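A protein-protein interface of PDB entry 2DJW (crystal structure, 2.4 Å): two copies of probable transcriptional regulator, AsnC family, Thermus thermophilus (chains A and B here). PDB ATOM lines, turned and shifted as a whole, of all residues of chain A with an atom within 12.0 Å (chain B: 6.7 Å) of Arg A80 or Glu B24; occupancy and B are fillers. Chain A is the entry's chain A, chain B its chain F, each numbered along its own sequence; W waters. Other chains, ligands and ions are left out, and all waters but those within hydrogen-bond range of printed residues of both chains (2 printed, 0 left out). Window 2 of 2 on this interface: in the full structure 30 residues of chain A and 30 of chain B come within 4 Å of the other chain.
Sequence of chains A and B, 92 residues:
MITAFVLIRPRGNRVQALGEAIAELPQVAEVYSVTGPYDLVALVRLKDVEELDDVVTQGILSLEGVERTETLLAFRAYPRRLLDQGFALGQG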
ATOM      1  N   ARG A  76      -9.939  37.515   6.250  1.00  0.00           N
ATOM      2  CA  ARG A  76     -10.182  37.007   4.910  1.00  0.00           C
ATOM      3  C   ARG A  76     -11.040  35.746   4.898  1.00  0.00           C
ATOM      4  O   ARG A  76     -10.730  34.777   5.584  1.00  0.00           O
ATOM      5  CB  ARG A  76      -8.852  36.763   4.186  1.00  0.00           C
ATOM      6  CG  ARG A  76      -9.032  36.578   2.710  1.00  0.00           C
ATOM      7  CD  ARG A  76      -7.898  35.774   2.146  1.00  0.00           C
ATOM      8  NE  ARG A  76      -8.256  35.095   0.897  1.00  0.00           N
ATOM      9  CZ  ARG A  76      -7.374  34.764  -0.039  1.00  0.00           C
ATOM     10  NH1 ARG A  76      -6.088  35.058   0.120  1.00  0.00           N
ATOM     11  NH2 ARG A  76      -7.783  34.127  -1.128  1.00  0.00           N
ATOM     12  N   ALA A  77     -12.116  35.787   4.112  1.00  0.00           N
ATOM     13  CA  ALA A  77     -12.973  34.637   3.843  1.00  0.00           C
ATOM     14  C   ALA A  77     -12.523  33.894   2.579  1.00  0.00           C
ATOM     15  O   ALA A  77     -12.110  34.523   1.603  1.00  0.00           O
ATOM     16  CB  ALA A  77     -14.397  35.089   3.695  1.00  0.00           C
ATOM     17  N   TYR A  78     -12.573  32.560   2.608  1.00  0.00           N
ATOM     18  CA  TYR A  78     -12.321  31.733   1.429  1.00  0.00           C
ATOM     19  C   TYR A  78     -13.655  31.147   0.963  1.00  0.00           C
ATOM     20  O   TYR A  78     -14.183  30.261   1.612  1.00  0.00           O
ATOM     21  CB  TYR A  78     -11.312  30.616   1.719  1.00  0.00           C
ATOM     22  CG  TYR A  78      -9.966  31.114   2.196  1.00  0.00           C
ATOM     23  CD1 TYR A  78      -8.937  31.366   1.291  1.00  0.00           C
ATOM     24  CD2 TYR A  78      -9.721  31.347   3.551  1.00  0.00           C
ATOM     25  CE1 TYR A  78      -7.714  31.850   1.715  1.00  0.00           C
ATOM     26  CE2 TYR A  78      -8.491  31.820   3.985  1.00  0.00           C
ATOM     27  CZ  TYR A  78      -7.489  32.069   3.068  1.00  0.00           C
ATOM     28  OH  TYR A  78      -6.254  32.537   3.489  1.00  0.00           O
ATOM     29  N   PRO A  79     -14.210  31.656  -0.156  1.00  0.00           N
ATOM     30  CA  PRO A  79     -15.527  31.256  -0.664  1.00  0.00           C
ATOM     31  C   PRO A  79     -15.607  29.864  -1.298  1.00  0.00           C
ATOM     32  O   PRO A  79     -14.621  29.114  -1.313  1.00  0.00           O
ATOM     33  CB  PRO A  79     -15.804  32.305  -1.744  1.00  0.00           C
ATOM     34  CG  PRO A  79     -14.473  32.668  -2.247  1.00  0.00           C
ATOM     35  CD  PRO A  79     -13.605  32.695  -1.014  1.00  0.00           C
ATOM     36  N   ARG A  80     -16.796  29.570  -1.837  1.00  0.00           N
ATOM     37  CA  ARG A  80     -17.171  28.311  -2.506  1.00  0.00           C
ATOM     38  C   ARG A  80     -17.540  27.221  -1.509  1.00  0.00           C
ATOM     39  O   ARG A  80     -17.585  27.513  -0.304  1.00  0.00           O
ATOM     40  CB  ARG A  80     -16.146  27.846  -3.551  1.00  0.00           C
ATOM     41  CG  ARG A  80     -16.394  28.436  -4.942  1.00  0.00           C
ATOM     42  CD  ARG A  80     -15.574  27.711  -6.019  1.00  0.00           C
ATOM     43  NE  ARG A  80     -16.138  26.410  -6.401  1.00  0.00           N
ATOM     44  CZ  ARG A  80     -15.414  25.353  -6.789  1.00  0.00           C
ATOM     45  NH1 ARG A  80     -14.083  25.421  -6.832  1.00  0.00           N
ATOM     46  NH2 ARG A  80     -16.018  24.212  -7.113  1.00  0.00           N
ATOM     47  N   GLY B  19      -6.602  27.170   2.951  1.00  0.00           N
ATOM     48  CA  GLY B  19      -7.839  27.914   3.071  1.00  0.00           C
ATOM     49  C   GLY B  19      -8.822  27.582   1.974  1.00  0.00           C
ATOM     50  O   GLY B  19      -9.980  27.279   2.244  1.00  0.00           O
ATOM     51  N   GLU B  20      -8.355  27.622   0.725  1.00  0.00           N
ATOM     52  CA  GLU B  20      -9.216  27.400  -0.442  1.00  0.00           C
ATOM     53  C   GLU B  20      -9.680  25.967  -0.571  1.00  0.00           C
ATOM     54  O   GLU B  20     -10.823  25.722  -0.936  1.00  0.00           O
ATOM     55  CB  GLU B  20      -8.489  27.842  -1.714  1.00  0.00           C
ATOM     56  CG  GLU B  20      -8.299  29.345  -1.777  1.00  0.00           C
ATOM     57  CD  GLU B  20      -7.394  29.768  -2.908  1.00  0.00           C
ATOM     58  OE1 GLU B  20      -7.445  30.958  -3.256  1.00  0.00           O
ATOM     59  OE2 GLU B  20      -6.644  28.919  -3.446  1.00  0.00           O
ATOM     60  N   ALA B  21      -8.777  25.038  -0.258  1.00  0.00           N
ATOM     61  CA  ALA B  21      -9.074  23.610  -0.182  1.00  0.00           C
ATOM     62  C   ALA B  21     -10.110  23.231   0.885  1.00  0.00           C
ATOM     63  O   ALA B  21     -10.962  22.394   0.615  1.00  0.00           O
ATOM     64  CB  ALA B  21      -7.783  22.825   0.038  1.00  0.00           C
ATOM     65  N   ILE B  22     -10.015  23.823   2.091  1.00  0.00           N
ATOM     66  CA  ILE B  22     -10.955  23.557   3.201  1.00  0.00           C
ATOM     67  C   ILE B  22     -12.345  24.066   2.822  1.00  0.00           C
ATOM     68  O   ILE B  22     -13.362  23.459   3.160  1.00  0.00           O
ATOM     69  CB  ILE B  22     -10.531  24.241   4.556  1.00  0.00           C
ATOM     70  CG1 ILE B  22      -9.084  23.929   4.988  1.00  0.00           C
ATOM     71  CG2 ILE B  22     -11.501  23.918   5.679  1.00  0.00           C
ATOM     72  CD1 ILE B  22      -8.705  22.522   4.971  1.00  0.00           C
ATOM     73  N   ALA B  23     -12.386  25.186   2.111  1.00  0.00           N
ATOM     74  CA  ALA B  23     -13.638  25.724   1.610  1.00  0.00           C
ATOM     75  C   ALA B  23     -14.349  24.818   0.585  1.00  0.00           C
ATOM     76  O   ALA B  23     -15.546  25.000   0.332  1.00  0.00           O
ATOM     77  CB  ALA B  23     -13.412  27.110   1.032  1.00  0.00           C
ATOM     78  N   GLU B  24     -13.635  23.861  -0.008  1.00  0.00           N
ATOM     79  CA  GLU B  24     -14.268  22.944  -0.980  1.00  0.00           C
ATOM     80  C   GLU B  24     -15.017  21.782  -0.329  1.00  0.00           C
ATOM     81  O   GLU B  24     -15.945  21.229  -0.923  1.00  0.00           O
ATOM     82  CB  GLU B  24     -13.274  22.433  -2.046  1.00  0.00           C
ATOM     83  CG  GLU B  24     -12.733  23.497  -3.036  1.00  0.00           C
ATOM     84  CD  GLU B  24     -13.702  24.683  -3.270  1.00  0.00           C
ATOM     85  OE1 GLU B  24     -14.886  24.452  -3.593  1.00  0.00           O
ATOM     86  OE2 GLU B  24     -13.270  25.854  -3.121  1.00  0.00           O
ATOM     87  N   LEU B  25     -14.610  21.429   0.893  1.00  0.00           N
ATOM     88  CA  LEU B  25     -15.264  20.384   1.714  1.00  0.00           C
ATOM     89  C   LEU B  25     -16.757  20.636   1.997  1.00  0.00           C
ATOM     90  O   LEU B  25     -17.131  21.708   2.462  1.00  0.00           O
ATOM     91  CB  LEU B  25     -14.526  20.198   3.044  1.00  0.00           C
ATOM     92  CG  LEU B  25     -13.045  19.857   2.988  1.00  0.00           C
ATOM     93  CD1 LEU B  25     -12.459  19.824   4.397  1.00  0.00           C
ATOM     94  CD2 LEU B  25     -12.830  18.546   2.225  1.00  0.00           C
ATOM     95  N   PRO B  26     -17.604  19.623   1.732  1.00  0.00           N
ATOM     96  CA  PRO B  26     -19.078  19.753   1.826  1.00  0.00           C
ATOM     97  C   PRO B  26     -19.605  20.258   3.190  1.00  0.00           C
ATOM     98  O   PRO B  26     -20.623  20.945   3.237  1.00  0.00           O
ATOM     99  CB  PRO B  26     -19.598  18.330   1.562  1.00  0.00           C
ATOM    100  CG  PRO B  26     -18.418  17.505   1.115  1.00  0.00           C
ATOM    101  CD  PRO B  26     -17.153  18.272   1.320  1.00  0.00           C
ATOM    102  N   GLN B  27     -18.916  19.926   4.275  1.00  0.00           N
ATOM    103  CA  GLN B  27     -19.401  20.232   5.622  1.00  0.00           C
ATOM    104  C   GLN B  27     -19.036  21.636   6.118  1.00  0.00           C
ATOM    105  O   GLN B  27     -19.576  22.097   7.122  1.00  0.00           O
ATOM    106  CB  GLN B  27     -18.910  19.175   6.609  1.00  0.00           C
ATOM    107  CG  GLN B  27     -19.272  17.750   6.215  1.00  0.00           C
ATOM    108  CD  GLN B  27     -18.267  17.083   5.279  1.00  0.00           C
ATOM    109  OE1 GLN B  27     -17.186  17.621   4.965  1.00  0.00           O
ATOM    110  NE2 GLN B  27     -18.623  15.886   4.831  1.00  0.00           N
ATOM    111  N   VAL B  28     -18.139  22.309   5.390  1.00  0.00           N
ATOM    112  CA  VAL B  28     -17.607  23.636   5.748  1.00  0.00           C
ATOM    113  C   VAL B  28     -18.494  24.753   5.227  1.00  0.00           C
ATOM    114  O   VAL B  28     -18.553  24.990   4.013  1.00  0.00           O
ATOM    115  CB  VAL B  28     -16.172  23.821   5.175  1.00  0.00           C
ATOM    116  CG1 VAL B  28     -15.680  25.253   5.357  1.00  0.00           C
ATOM    117  CG2 VAL B  28     -15.190  22.805   5.802  1.00  0.00           C
ATOM    118  N   ALA B  29     -19.178  25.444   6.136  1.00  0.00           N
ATOM    119  CA  ALA B  29     -20.066  26.530   5.742  1.00  0.00           C
ATOM    120  C   ALA B  29     -19.315  27.849   5.588  1.00  0.00           C
ATOM    121  O   ALA B  29     -19.697  28.700   4.775  1.00  0.00           O
ATOM    122  CB  ALA B  29     -21.212  26.678   6.737  1.00  0.00           C
ATOM    123  N   VAL B  31     -15.066  29.495   6.188  1.00  0.00           N
ATOM    124  CA  VAL B  31     -13.680  29.269   6.570  1.00  0.00           C
ATOM    125  C   VAL B  31     -12.909  30.560   6.393  1.00  0.00           C
ATOM    126  O   VAL B  31     -13.103  31.277   5.415  1.00  0.00           O
ATOM    127  CB  VAL B  31     -13.027  28.043   5.867  1.00  0.00           C
ATOM    128  CG1 VAL B  31     -13.146  28.127   4.369  1.00  0.00           C
ATOM    129  CG2 VAL B  31     -11.563  27.847   6.330  1.00  0.00           C
HETATM  130  O   HOH W   1     -16.014  30.914   3.794  1.00  0.00           O
HETATM  131  O   HOH W   2      -9.758  32.236  -2.598  1.00  0.00           O
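Along chain A the printed residues that touch a printed residue of chain B span positions 76 to 80.
Of the 12 printed residues of chain B, 5 touch a printed residue of chain A.
Among the printed residues, Asp or Glu carboxylates within 4 Å of a Lys or Arg side-chain nitrogen of the other chain: Arg A76 with Glu B20 (3.8 Å) and Arg A80 with Glu B24 (3.5 Å).
Water W2 bridges the side-chain carboxylate of Glu B20 (2.7 Å) and the guanidinium group of Arg A76 (3.1 Å).
Water W1 bridges O of Tyr A78 (2.9 Å) and N of Val B31 (2.9 Å).
No position is printed for both chains.
Of the 10 pairs that touch across the chains among the printed residues, none has its exchanged pair printed and touching as well.
The guanidinium group (NH2) of Arg A76 lies within salt-bridge range of the side-chain carboxylate (OE1) of Glu B20, at 3.8 Å.
The backbone NH (N) of Tyr A78 is in hydrogen-bond range of the backbone carbonyl oxygen (O) of Val B31.
The guanidinium group (NH1) of Arg A80 lies within salt-bridge range of the side-chain carboxylate (OE1) of Glu B24 (3.5 Å).
The backbone carbonyl oxygen (O) of Arg A80 lies close to the backbone carbonyl oxygen (O) of Ala B23, 3.3 Å away.
Arg A80 touches just these residues of chain B: Ala B23 (3.3 Å) and Glu B24 (3.4 Å).
Glu B24 touches just these residues of chain A: Pro A79 (3.97 Å) and Arg A80 (3.4 Å).
Of chain A, only Arg A76 and Tyr A78 come within 4 Å of Glu B20.
No residue of chain A comes within 4 Å of Leu B25.
No residue of chain A comes within 4 Å of Pro B26.
No residue of chain A comes within 4 Å of Val B28.
Printed residues of chain B within 4 Å of Ala A77: Val B31.
Of the printed residues of chain B, Pro A79 touches Ala B23 (3.3 Å) and Glu B24 (3.97 Å).
Printed residues of chain A within 4 Å of Gly B19: Tyr A78.
The nearest residue of chain B that does not touch Arg A80 is Val B28 (5.1 Å).
Ala A77 touches Val B31 (CA to O, 3.7 Å).
Tyr A78 touches Gly B19 (CB to O, 3.6 Å).
Glu B20 touches Tyr A78.
Tyr A78 touches Ala B23.
Pro A79 touches Ala B23.
O of Pro A79 touches OE2 of Glu B24 (3.97 Å).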
